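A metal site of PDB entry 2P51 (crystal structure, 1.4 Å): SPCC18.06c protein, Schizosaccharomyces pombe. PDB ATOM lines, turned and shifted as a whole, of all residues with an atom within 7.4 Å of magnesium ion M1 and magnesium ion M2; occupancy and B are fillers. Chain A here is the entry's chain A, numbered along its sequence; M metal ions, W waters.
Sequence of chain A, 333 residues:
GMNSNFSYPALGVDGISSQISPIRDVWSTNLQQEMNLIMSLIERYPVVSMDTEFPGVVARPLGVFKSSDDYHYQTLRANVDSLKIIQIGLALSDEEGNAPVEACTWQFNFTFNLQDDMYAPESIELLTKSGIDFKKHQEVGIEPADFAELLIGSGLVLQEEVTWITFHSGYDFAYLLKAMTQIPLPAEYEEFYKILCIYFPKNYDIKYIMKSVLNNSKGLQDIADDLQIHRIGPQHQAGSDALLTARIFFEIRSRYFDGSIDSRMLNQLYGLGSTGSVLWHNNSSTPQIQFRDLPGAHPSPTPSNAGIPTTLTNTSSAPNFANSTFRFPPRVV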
ATOM      1  N   MET A  50     -14.436  32.161  13.843  1.00  0.00           N
ATOM      2  CA  MET A  50     -13.148  31.594  14.249  1.00  0.00           C
ATOM      3  C   MET A  50     -13.242  30.081  14.394  1.00  0.00           C
ATOM      4  O   MET A  50     -14.294  29.541  14.792  1.00  0.00           O
ATOM      5  CB  MET A  50     -12.699  32.244  15.569  1.00  0.00           C
ATOM      6  CG  MET A  50     -11.418  31.740  16.185  1.00  0.00           C
ATOM      7  SD  MET A  50     -11.656  30.276  17.239  1.00  0.00           S
ATOM      8  CE  MET A  50     -12.369  31.090  18.694  1.00  0.00           C
ATOM      9  N   ASP A  51     -12.091  29.482  14.069  1.00  0.00           N
ATOM     10  CA  ASP A  51     -11.865  28.059  14.335  1.00  0.00           C
ATOM     11  C   ASP A  51     -10.397  27.848  14.710  1.00  0.00           C
ATOM     12  O   ASP A  51      -9.591  28.761  14.360  1.00  0.00           O
ATOM     13  CB  ASP A  51     -12.199  27.156  13.136  1.00  0.00           C
ATOM     14  CG  ASP A  51     -12.163  25.669  13.471  1.00  0.00           C
ATOM     15  OD1 ASP A  51     -12.525  25.324  14.631  1.00  0.00           O
ATOM     16  OD2 ASP A  51     -11.795  24.910  12.565  1.00  0.00           O
ATOM     17  N   THR A  52     -10.062  26.718  15.325  1.00  0.00           N
ATOM     18  CA  THR A  52      -8.641  26.441  15.531  1.00  0.00           C
ATOM     19  C   THR A  52      -8.369  24.971  15.186  1.00  0.00           C
ATOM     20  O   THR A  52      -9.282  24.151  15.186  1.00  0.00           O
ATOM     21  CB  THR A  52      -8.138  26.632  16.982  1.00  0.00           C
ATOM     22  OG1 THR A  52      -8.611  25.565  17.804  1.00  0.00           O
ATOM     23  CG2 THR A  52      -8.598  27.985  17.566  1.00  0.00           C
ATOM     24  N   GLU A  53      -7.132  24.640  14.832  1.00  0.00           N
ATOM     25  CA  GLU A  53      -6.742  23.247  14.747  1.00  0.00           C
ATOM     26  C   GLU A  53      -5.657  23.030  15.832  1.00  0.00           C
ATOM     27  O   GLU A  53      -4.828  23.912  16.102  1.00  0.00           O
ATOM     28  CB  GLU A  53      -6.192  22.864  13.381  1.00  0.00           C
ATOM     29  CG  GLU A  53      -7.099  23.150  12.187  1.00  0.00           C
ATOM     30  CD  GLU A  53      -8.449  22.494  12.254  1.00  0.00           C
ATOM     31  OE1 GLU A  53      -8.583  21.360  12.737  1.00  0.00           O
ATOM     32  OE2 GLU A  53      -9.438  23.153  11.798  1.00  0.00           O
ATOM     33  N   PHE A  54      -5.642  21.854  16.436  1.00  0.00           N
ATOM     34  CA  PHE A  54      -4.754  21.515  17.540  1.00  0.00           C
ATOM     35  C   PHE A  54      -4.647  19.993  17.565  1.00  0.00           C
ATOM     36  O   PHE A  54      -5.404  19.317  16.834  1.00  0.00           O
ATOM     37  CB  PHE A  54      -5.319  22.077  18.856  1.00  0.00           C
ATOM     38  CG  PHE A  54      -6.767  21.686  19.112  1.00  0.00           C
ATOM     39  CD1 PHE A  54      -7.080  20.482  19.755  1.00  0.00           C
ATOM     40  CD2 PHE A  54      -7.794  22.547  18.726  1.00  0.00           C
ATOM     41  CE1 PHE A  54      -8.396  20.139  19.992  1.00  0.00           C
ATOM     42  CE2 PHE A  54      -9.115  22.191  18.943  1.00  0.00           C
ATOM     43  CZ  PHE A  54      -9.392  20.981  19.586  1.00  0.00           C
ATOM     44  N   GLN A  87      -3.258  25.834  14.271  1.00  0.00           N
ATOM     45  CA  GLN A  87      -3.730  26.856  13.377  1.00  0.00           C
ATOM     46  C   GLN A  87      -4.875  27.658  14.050  1.00  0.00           C
ATOM     47  O   GLN A  87      -5.634  27.076  14.819  1.00  0.00           O
ATOM     48  CB  GLN A  87      -4.389  26.376  12.076  1.00  0.00           C
ATOM     49  CG  GLN A  87      -3.506  25.838  11.000  1.00  0.00           C
ATOM     50  CD  GLN A  87      -4.266  25.389   9.769  1.00  0.00           C
ATOM     51  OE1 GLN A  87      -5.384  24.827   9.907  1.00  0.00           O
ATOM     52  NE2 GLN A  87      -3.691  25.556   8.611  1.00  0.00           N
ATOM     53  N   LEU A 127      -4.651  15.796  10.338  1.00  0.00           N
ATOM     54  CA  LEU A 127      -4.245  17.131   9.855  1.00  0.00           C
ATOM     55  C   LEU A 127      -3.358  17.044   8.619  1.00  0.00           C
ATOM     56  O   LEU A 127      -3.409  17.840   7.676  1.00  0.00           O
ATOM     57  CB  LEU A 127      -3.540  17.895  11.005  1.00  0.00           C
ATOM     58  CG  LEU A 127      -4.519  18.379  12.090  1.00  0.00           C
ATOM     59  CD1 LEU A 127      -3.787  18.793  13.362  1.00  0.00           C
ATOM     60  CD2 LEU A 127      -5.426  19.535  11.604  1.00  0.00           C
ATOM     61  N   THR A 166     -18.547  31.288  16.502  1.00  0.00           N
ATOM     62  CA  THR A 166     -17.767  30.050  16.678  1.00  0.00           C
ATOM     63  C   THR A 166     -18.693  28.872  16.489  1.00  0.00           C
ATOM     64  O   THR A 166     -19.903  29.047  16.274  1.00  0.00           O
ATOM     65  CB  THR A 166     -17.120  30.021  18.081  1.00  0.00           C
ATOM     66  OG1 THR A 166     -18.196  30.065  19.037  1.00  0.00           O
ATOM     67  CG2 THR A 166     -16.175  31.230  18.300  1.00  0.00           C
ATOM     68  N   PHE A 167     -18.113  27.664  16.574  1.00  0.00           N
ATOM     69  CA  PHE A 167     -18.947  26.452  16.505  1.00  0.00           C
ATOM     70  C   PHE A 167     -18.348  25.443  17.481  1.00  0.00           C
ATOM     71  O   PHE A 167     -17.178  25.017  17.286  1.00  0.00           O
ATOM     72  CB  PHE A 167     -18.984  25.912  15.077  1.00  0.00           C
ATOM     73  CG  PHE A 167     -19.855  24.660  14.938  1.00  0.00           C
ATOM     74  CD1 PHE A 167     -21.187  24.790  14.593  1.00  0.00           C
ATOM     75  CD2 PHE A 167     -19.305  23.373  15.144  1.00  0.00           C
ATOM     76  CE1 PHE A 167     -22.025  23.685  14.473  1.00  0.00           C
ATOM     77  CE2 PHE A 167     -20.139  22.282  15.094  1.00  0.00           C
ATOM     78  CZ  PHE A 167     -21.474  22.443  14.759  1.00  0.00           C
ATOM     79  N   HIS A 168     -19.120  25.010  18.489  1.00  0.00           N
ATOM     80  CA  HIS A 168     -18.684  23.994  19.464  1.00  0.00           C
ATOM     81  C   HIS A 168     -17.340  24.419  20.037  1.00  0.00           C
ATOM     82  O   HIS A 168     -16.285  23.787  19.883  1.00  0.00           O
ATOM     83  CB  HIS A 168     -18.631  22.620  18.809  1.00  0.00           C
ATOM     84  CG  HIS A 168     -18.745  21.464  19.752  1.00  0.00           C
ATOM     85  ND1 HIS A 168     -18.350  21.506  21.073  1.00  0.00           N
ATOM     86  CD2 HIS A 168     -19.231  20.211  19.544  1.00  0.00           C
ATOM     87  CE1 HIS A 168     -18.585  20.327  21.636  1.00  0.00           C
ATOM     88  NE2 HIS A 168     -19.123  19.507  20.707  1.00  0.00           N
ATOM     89  N   SER A 169     -17.393  25.573  20.674  1.00  0.00           N
ATOM     90  CA  SER A 169     -16.276  26.475  20.785  1.00  0.00           C
ATOM     91  C   SER A 169     -15.390  26.333  22.018  1.00  0.00           C
ATOM     92  O   SER A 169     -14.474  27.144  22.139  1.00  0.00           O
ATOM     93  CB  SER A 169     -16.792  27.953  20.798  1.00  0.00           C
ATOM     94  OG  SER A 169     -17.611  28.060  21.985  1.00  0.00           O
ATOM     95  N   GLY A 170     -15.613  25.391  22.940  1.00  0.00           N
ATOM     96  CA  GLY A 170     -14.849  25.370  24.203  1.00  0.00           C
ATOM     97  C   GLY A 170     -13.346  25.325  23.948  1.00  0.00           C
ATOM     98  O   GLY A 170     -12.579  26.126  24.488  1.00  0.00           O
ATOM     99  N   TYR A 171     -12.901  24.348  23.163  1.00  0.00           N
ATOM    100  CA  TYR A 171     -11.463  24.252  22.908  1.00  0.00           C
ATOM    101  C   TYR A 171     -10.958  25.444  22.106  1.00  0.00           C
ATOM    102  O   TYR A 171      -9.870  25.949  22.418  1.00  0.00           O
ATOM    103  CB  TYR A 171     -11.076  22.942  22.154  1.00  0.00           C
ATOM    104  CG  TYR A 171     -11.000  21.729  23.048  1.00  0.00           C
ATOM    105  CD1 TYR A 171     -12.158  21.108  23.566  1.00  0.00           C
ATOM    106  CD2 TYR A 171      -9.775  21.133  23.384  1.00  0.00           C
ATOM    107  CE1 TYR A 171     -12.087  19.980  24.379  1.00  0.00           C
ATOM    108  CE2 TYR A 171      -9.727  20.006  24.197  1.00  0.00           C
ATOM    109  CZ  TYR A 171     -10.857  19.419  24.695  1.00  0.00           C
ATOM    110  OH  TYR A 171     -10.809  18.292  25.509  1.00  0.00           O
ATOM    111  N   ASP A 172     -11.682  25.835  21.072  1.00  0.00           N
ATOM    112  CA  ASP A 172     -11.235  26.912  20.191  1.00  0.00           C
ATOM    113  C   ASP A 172     -11.023  28.208  20.977  1.00  0.00           C
ATOM    114  O   ASP A 172      -9.981  28.889  20.869  1.00  0.00           O
ATOM    115  CB  ASP A 172     -12.259  27.068  19.067  1.00  0.00           C
ATOM    116  CG  ASP A 172     -12.316  25.962  18.060  1.00  0.00           C
ATOM    117  OD1 ASP A 172     -11.283  25.233  17.986  1.00  0.00           O
ATOM    118  OD2 ASP A 172     -13.325  25.721  17.367  1.00  0.00           O
ATOM    119  N   LEU A 220     -20.798  20.990  11.776  1.00  0.00           N
ATOM    120  CA  LEU A 220     -20.640  22.123  10.893  1.00  0.00           C
ATOM    121  C   LEU A 220     -20.809  21.775   9.424  1.00  0.00           C
ATOM    122  O   LEU A 220     -21.552  22.401   8.669  1.00  0.00           O
ATOM    123  CB  LEU A 220     -19.214  22.682  11.136  1.00  0.00           C
ATOM    124  CG  LEU A 220     -18.929  23.994  10.423  1.00  0.00           C
ATOM    125  CD1 LEU A 220     -19.723  25.163  11.017  1.00  0.00           C
ATOM    126  CD2 LEU A 220     -17.439  24.340  10.497  1.00  0.00           C
ATOM    127  N   ARG A 231     -18.405  25.086   0.711  1.00  0.00           N
ATOM    128  CA  ARG A 231     -17.124  25.285   1.315  1.00  0.00           C
ATOM    129  C   ARG A 231     -16.087  25.739   0.297  1.00  0.00           C
ATOM    130  O   ARG A 231     -15.921  25.183  -0.790  1.00  0.00           O
ATOM    131  CB  ARG A 231     -16.631  23.975   1.961  1.00  0.00           C
ATOM    132  CG  ARG A 231     -15.260  24.171   2.615  1.00  0.00           C
ATOM    133  CD  ARG A 231     -14.753  22.855   3.161  1.00  0.00           C
ATOM    134  NE  ARG A 231     -15.351  22.425   4.440  1.00  0.00           N
ATOM    135  CZ  ARG A 231     -15.008  22.850   5.640  1.00  0.00           C
ATOM    136  NH1 ARG A 231     -14.060  23.785   5.830  1.00  0.00           N
ATOM    137  NH2 ARG A 231     -15.650  22.322   6.680  1.00  0.00           N
ATOM    138  N   PRO A 234     -10.013  23.714   2.075  1.00  0.00           N
ATOM    139  CA  PRO A 234      -9.972  22.362   2.629  1.00  0.00           C
ATOM    140  C   PRO A 234     -10.700  22.193   3.967  1.00  0.00           C
ATOM    141  O   PRO A 234     -10.446  22.938   4.906  1.00  0.00           O
ATOM    142  CB  PRO A 234      -8.456  22.117   2.815  1.00  0.00           C
ATOM    143  CG  PRO A 234      -7.845  23.481   2.893  1.00  0.00           C
ATOM    144  CD  PRO A 234      -8.732  24.448   2.177  1.00  0.00           C
ATOM    145  N   GLN A 235     -11.584  21.188   4.077  1.00  0.00           N
ATOM    146  CA  GLN A 235     -12.162  20.812   5.366  1.00  0.00           C
ATOM    147  C   GLN A 235     -11.047  20.454   6.351  1.00  0.00           C
ATOM    148  O   GLN A 235     -10.008  19.859   6.037  1.00  0.00           O
ATOM    149  CB  GLN A 235     -13.132  19.657   5.157  1.00  0.00           C
ATOM    150  CG  GLN A 235     -13.884  19.180   6.376  1.00  0.00           C
ATOM    151  CD  GLN A 235     -15.063  18.293   6.054  1.00  0.00           C
ATOM    152  OE1 GLN A 235     -15.813  17.957   6.983  1.00  0.00           O
ATOM    153  NE2 GLN A 235     -15.286  17.845   4.825  1.00  0.00           N
ATOM    154  N   HIS A 236     -11.275  20.829   7.619  1.00  0.00           N
ATOM    155  CA  HIS A 236     -10.361  20.480   8.694  1.00  0.00           C
ATOM    156  C   HIS A 236      -9.077  21.281   8.536  1.00  0.00           C
ATOM    157  O   HIS A 236      -8.035  20.822   9.011  1.00  0.00           O
ATOM    158  CB  HIS A 236     -10.160  18.946   8.749  1.00  0.00           C
ATOM    159  CG  HIS A 236      -9.791  18.538  10.132  1.00  0.00           C
ATOM    160  ND1 HIS A 236     -10.727  18.008  11.000  1.00  0.00           N
ATOM    161  CD2 HIS A 236      -8.610  18.594  10.796  1.00  0.00           C
ATOM    162  CE1 HIS A 236     -10.133  17.756  12.173  1.00  0.00           C
ATOM    163  NE2 HIS A 236      -8.835  18.091  12.076  1.00  0.00           N
ATOM    164  N   GLN A 237      -9.177  22.473   7.931  1.00  0.00           N
ATOM    165  CA  GLN A 237      -8.154  23.486   8.052  1.00  0.00           C
ATOM    166  C   GLN A 237      -8.843  24.736   8.626  1.00  0.00           C
ATOM    167  O   GLN A 237      -9.986  24.984   8.211  1.00  0.00           O
ATOM    168  CB  GLN A 237      -7.372  23.802   6.753  1.00  0.00           C
ATOM    169  CG  GLN A 237      -6.405  22.614   6.471  1.00  0.00           C
ATOM    170  CD  GLN A 237      -5.200  23.035   5.673  1.00  0.00           C
ATOM    171  OE1 GLN A 237      -4.493  23.994   5.973  1.00  0.00           O
ATOM    172  NE2 GLN A 237      -4.896  22.345   4.557  1.00  0.00           N
ATOM    173  N   ALA A 238      -8.188  25.443   9.546  1.00  0.00           N
ATOM    174  CA  ALA A 238      -8.959  26.415  10.340  1.00  0.00           C
ATOM    175  C   ALA A 238      -9.462  27.577   9.504  1.00  0.00           C
ATOM    176  O   ALA A 238     -10.530  28.116   9.799  1.00  0.00           O
ATOM    177  CB  ALA A 238      -8.183  26.926  11.521  1.00  0.00           C
ATOM    178  N   GLY A 239      -8.739  28.021   8.476  1.00  0.00           N
ATOM    179  CA  GLY A 239      -9.178  29.114   7.641  1.00  0.00           C
ATOM    180  C   GLY A 239     -10.481  28.795   6.967  1.00  0.00           C
ATOM    181  O   GLY A 239     -11.487  29.536   7.061  1.00  0.00           O
ATOM    182  N   SER A 240     -10.558  27.659   6.290  1.00  0.00           N
ATOM    183  CA  SER A 240     -11.749  27.214   5.588  1.00  0.00           C
ATOM    184  C   SER A 240     -12.873  26.929   6.565  1.00  0.00           C
ATOM    185  O   SER A 240     -14.026  27.317   6.320  1.00  0.00           O
ATOM    186  CB  SER A 240     -11.374  25.953   4.783  1.00  0.00           C
ATOM    187  OG  SER A 240     -12.531  25.458   4.130  1.00  0.00           O
ATOM    188  N   ASP A 241     -12.544  26.271   7.678  1.00  0.00           N
ATOM    189  CA  ASP A 241     -13.615  25.988   8.655  1.00  0.00           C
ATOM    190  C   ASP A 241     -14.185  27.291   9.239  1.00  0.00           C
ATOM    191  O   ASP A 241     -15.422  27.379   9.445  1.00  0.00           O
ATOM    192  CB  ASP A 241     -13.102  25.117   9.780  1.00  0.00           C
ATOM    193  CG  ASP A 241     -12.693  23.708   9.385  1.00  0.00           C
ATOM    194  OD1 ASP A 241     -13.111  23.206   8.306  1.00  0.00           O
ATOM    195  OD2 ASP A 241     -11.929  23.037  10.140  1.00  0.00           O
ATOM    196  N   ALA A 242     -13.361  28.281   9.499  1.00  0.00           N
ATOM    197  CA  ALA A 242     -13.851  29.554  10.043  1.00  0.00           C
ATOM    198  C   ALA A 242     -14.725  30.251   9.028  1.00  0.00           C
ATOM    199  O   ALA A 242     -15.753  30.896   9.312  1.00  0.00           O
ATOM    200  CB  ALA A 242     -12.659  30.459  10.404  1.00  0.00           C
ATOM    201  N   THR A 245     -18.067  28.615   8.952  1.00  0.00           N
ATOM    202  CA  THR A 245     -18.745  29.039  10.158  1.00  0.00           C
ATOM    203  C   THR A 245     -19.427  30.375   9.921  1.00  0.00           C
ATOM    204  O   THR A 245     -20.625  30.547  10.257  1.00  0.00           O
ATOM    205  CB  THR A 245     -17.746  29.156  11.321  1.00  0.00           C
ATOM    206  OG1 THR A 245     -17.217  27.817  11.577  1.00  0.00           O
ATOM    207  CG2 THR A 245     -18.397  29.592  12.627  1.00  0.00           C
HETATM  208 MG    MG M   1     -11.485  22.896  12.132  1.00  0.00          MG
HETATM  209 MG    MG M   2     -13.699  24.227  15.910  1.00  0.00          MG
HETATM  210  O   HOH W   1     -11.123  22.477  14.185  1.00  0.00           O
HETATM  211  O   HOH W   2     -11.088  20.857  11.920  1.00  0.00           O
HETATM  212  O   HOH W   3     -13.877  22.833  14.484  1.00  0.00           O
HETATM  213  O   HOH W   4     -12.142  23.114  16.679  1.00  0.00           O
HETATM  214  O   HOH W   5     -15.447  25.156  15.332  1.00  0.00           O
HETATM  215  O   HOH W   6     -15.024  23.172  17.199  1.00  0.00           O
HETATM  216  O   HOH W   7     -13.538  22.483  12.286  1.00  0.00           O
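The side-chain carboxylate (OD1) of Asp 241 lies within hydrogen-bond range of the backbone NH (N) of His 236, at 3.1 Å.
O of Asp 241 lies within hydrogen-bond range of OG1 of Thr 245.
The side-chain carboxylate (OD1) of Asp 241 lies within salt-bridge range of the guanidinium group (NH1) of Arg 231, 2.7 Å away.
OE1 of Glu 53 lies within hydrogen-bond range of NE2 of His 236, 3.3 Å away.
The side-chain carboxylate of Glu 53 sits close to the backbone NH of Ala 238 (3.4 Å).
The backbone NH (N) of Glu 53 sits at hydrogen-bond distance from the backbone carbonyl oxygen (O) of Gln 87 (2.9 Å).
OD1 of Asp 172 is in hydrogen-bond range of OG1 of Thr 52 (2.7 Å).
Merely in contact with magnesium ion M1: Thr 52.
Within 4 Å of magnesium ion M1: Asp 51, Thr 52, Glu 53 and Asp 241.
The nearest printed residue that does not touch magnesium ion M1 is His 236 (4.3 Å).
Merely in contact with magnesium ion M2: Phe 167 (3.8 Å).
Of the 26 residues printed, 3 come within 4 Å of magnesium ion M2.
The nearest printed residue that does not touch magnesium ion M2 is Thr 52 (4.4 Å).
Magnesium ion M2 is bound by water W3, 2.0 Å away.
OD1 of Asp 51 binds magnesium ion M2 (2.1 Å).
Water W5 is bound to magnesium ion M2 (2.1 Å).
Water W4 is bound to magnesium ion M2 (2.1 Å).
Magnesium ion M2 is bound by OD2 of Asp 172 (2.1 Å).
Water W6 binds magnesium ion M2, 2.1 Å away.
Magnesium ion M2 has six donor atoms within binding distance.
Water W2 lies within hydrogen-bond range of OE1 of Glu 53 (2.7 Å) and ND1 of His 236 (3.0 Å).
Water W1 bridges O of Thr 52 (2.7 Å) and OE1 of Glu 53 (3.1 Å).
Water W4 lies within hydrogen-bond range of OD1 of Asp 172 (2.6 Å) and O of Thr 52 (3.4 Å).
Magnesium ion M1 is bound by OD2 of Asp 241 (2.0 Å), OD2 of Asp 51 (2.1 Å), water W2 (2.1 Å), OE2 of Glu 53 (2.1 Å), water W7 (2.1 Å) and water W1 (2.1 Å).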
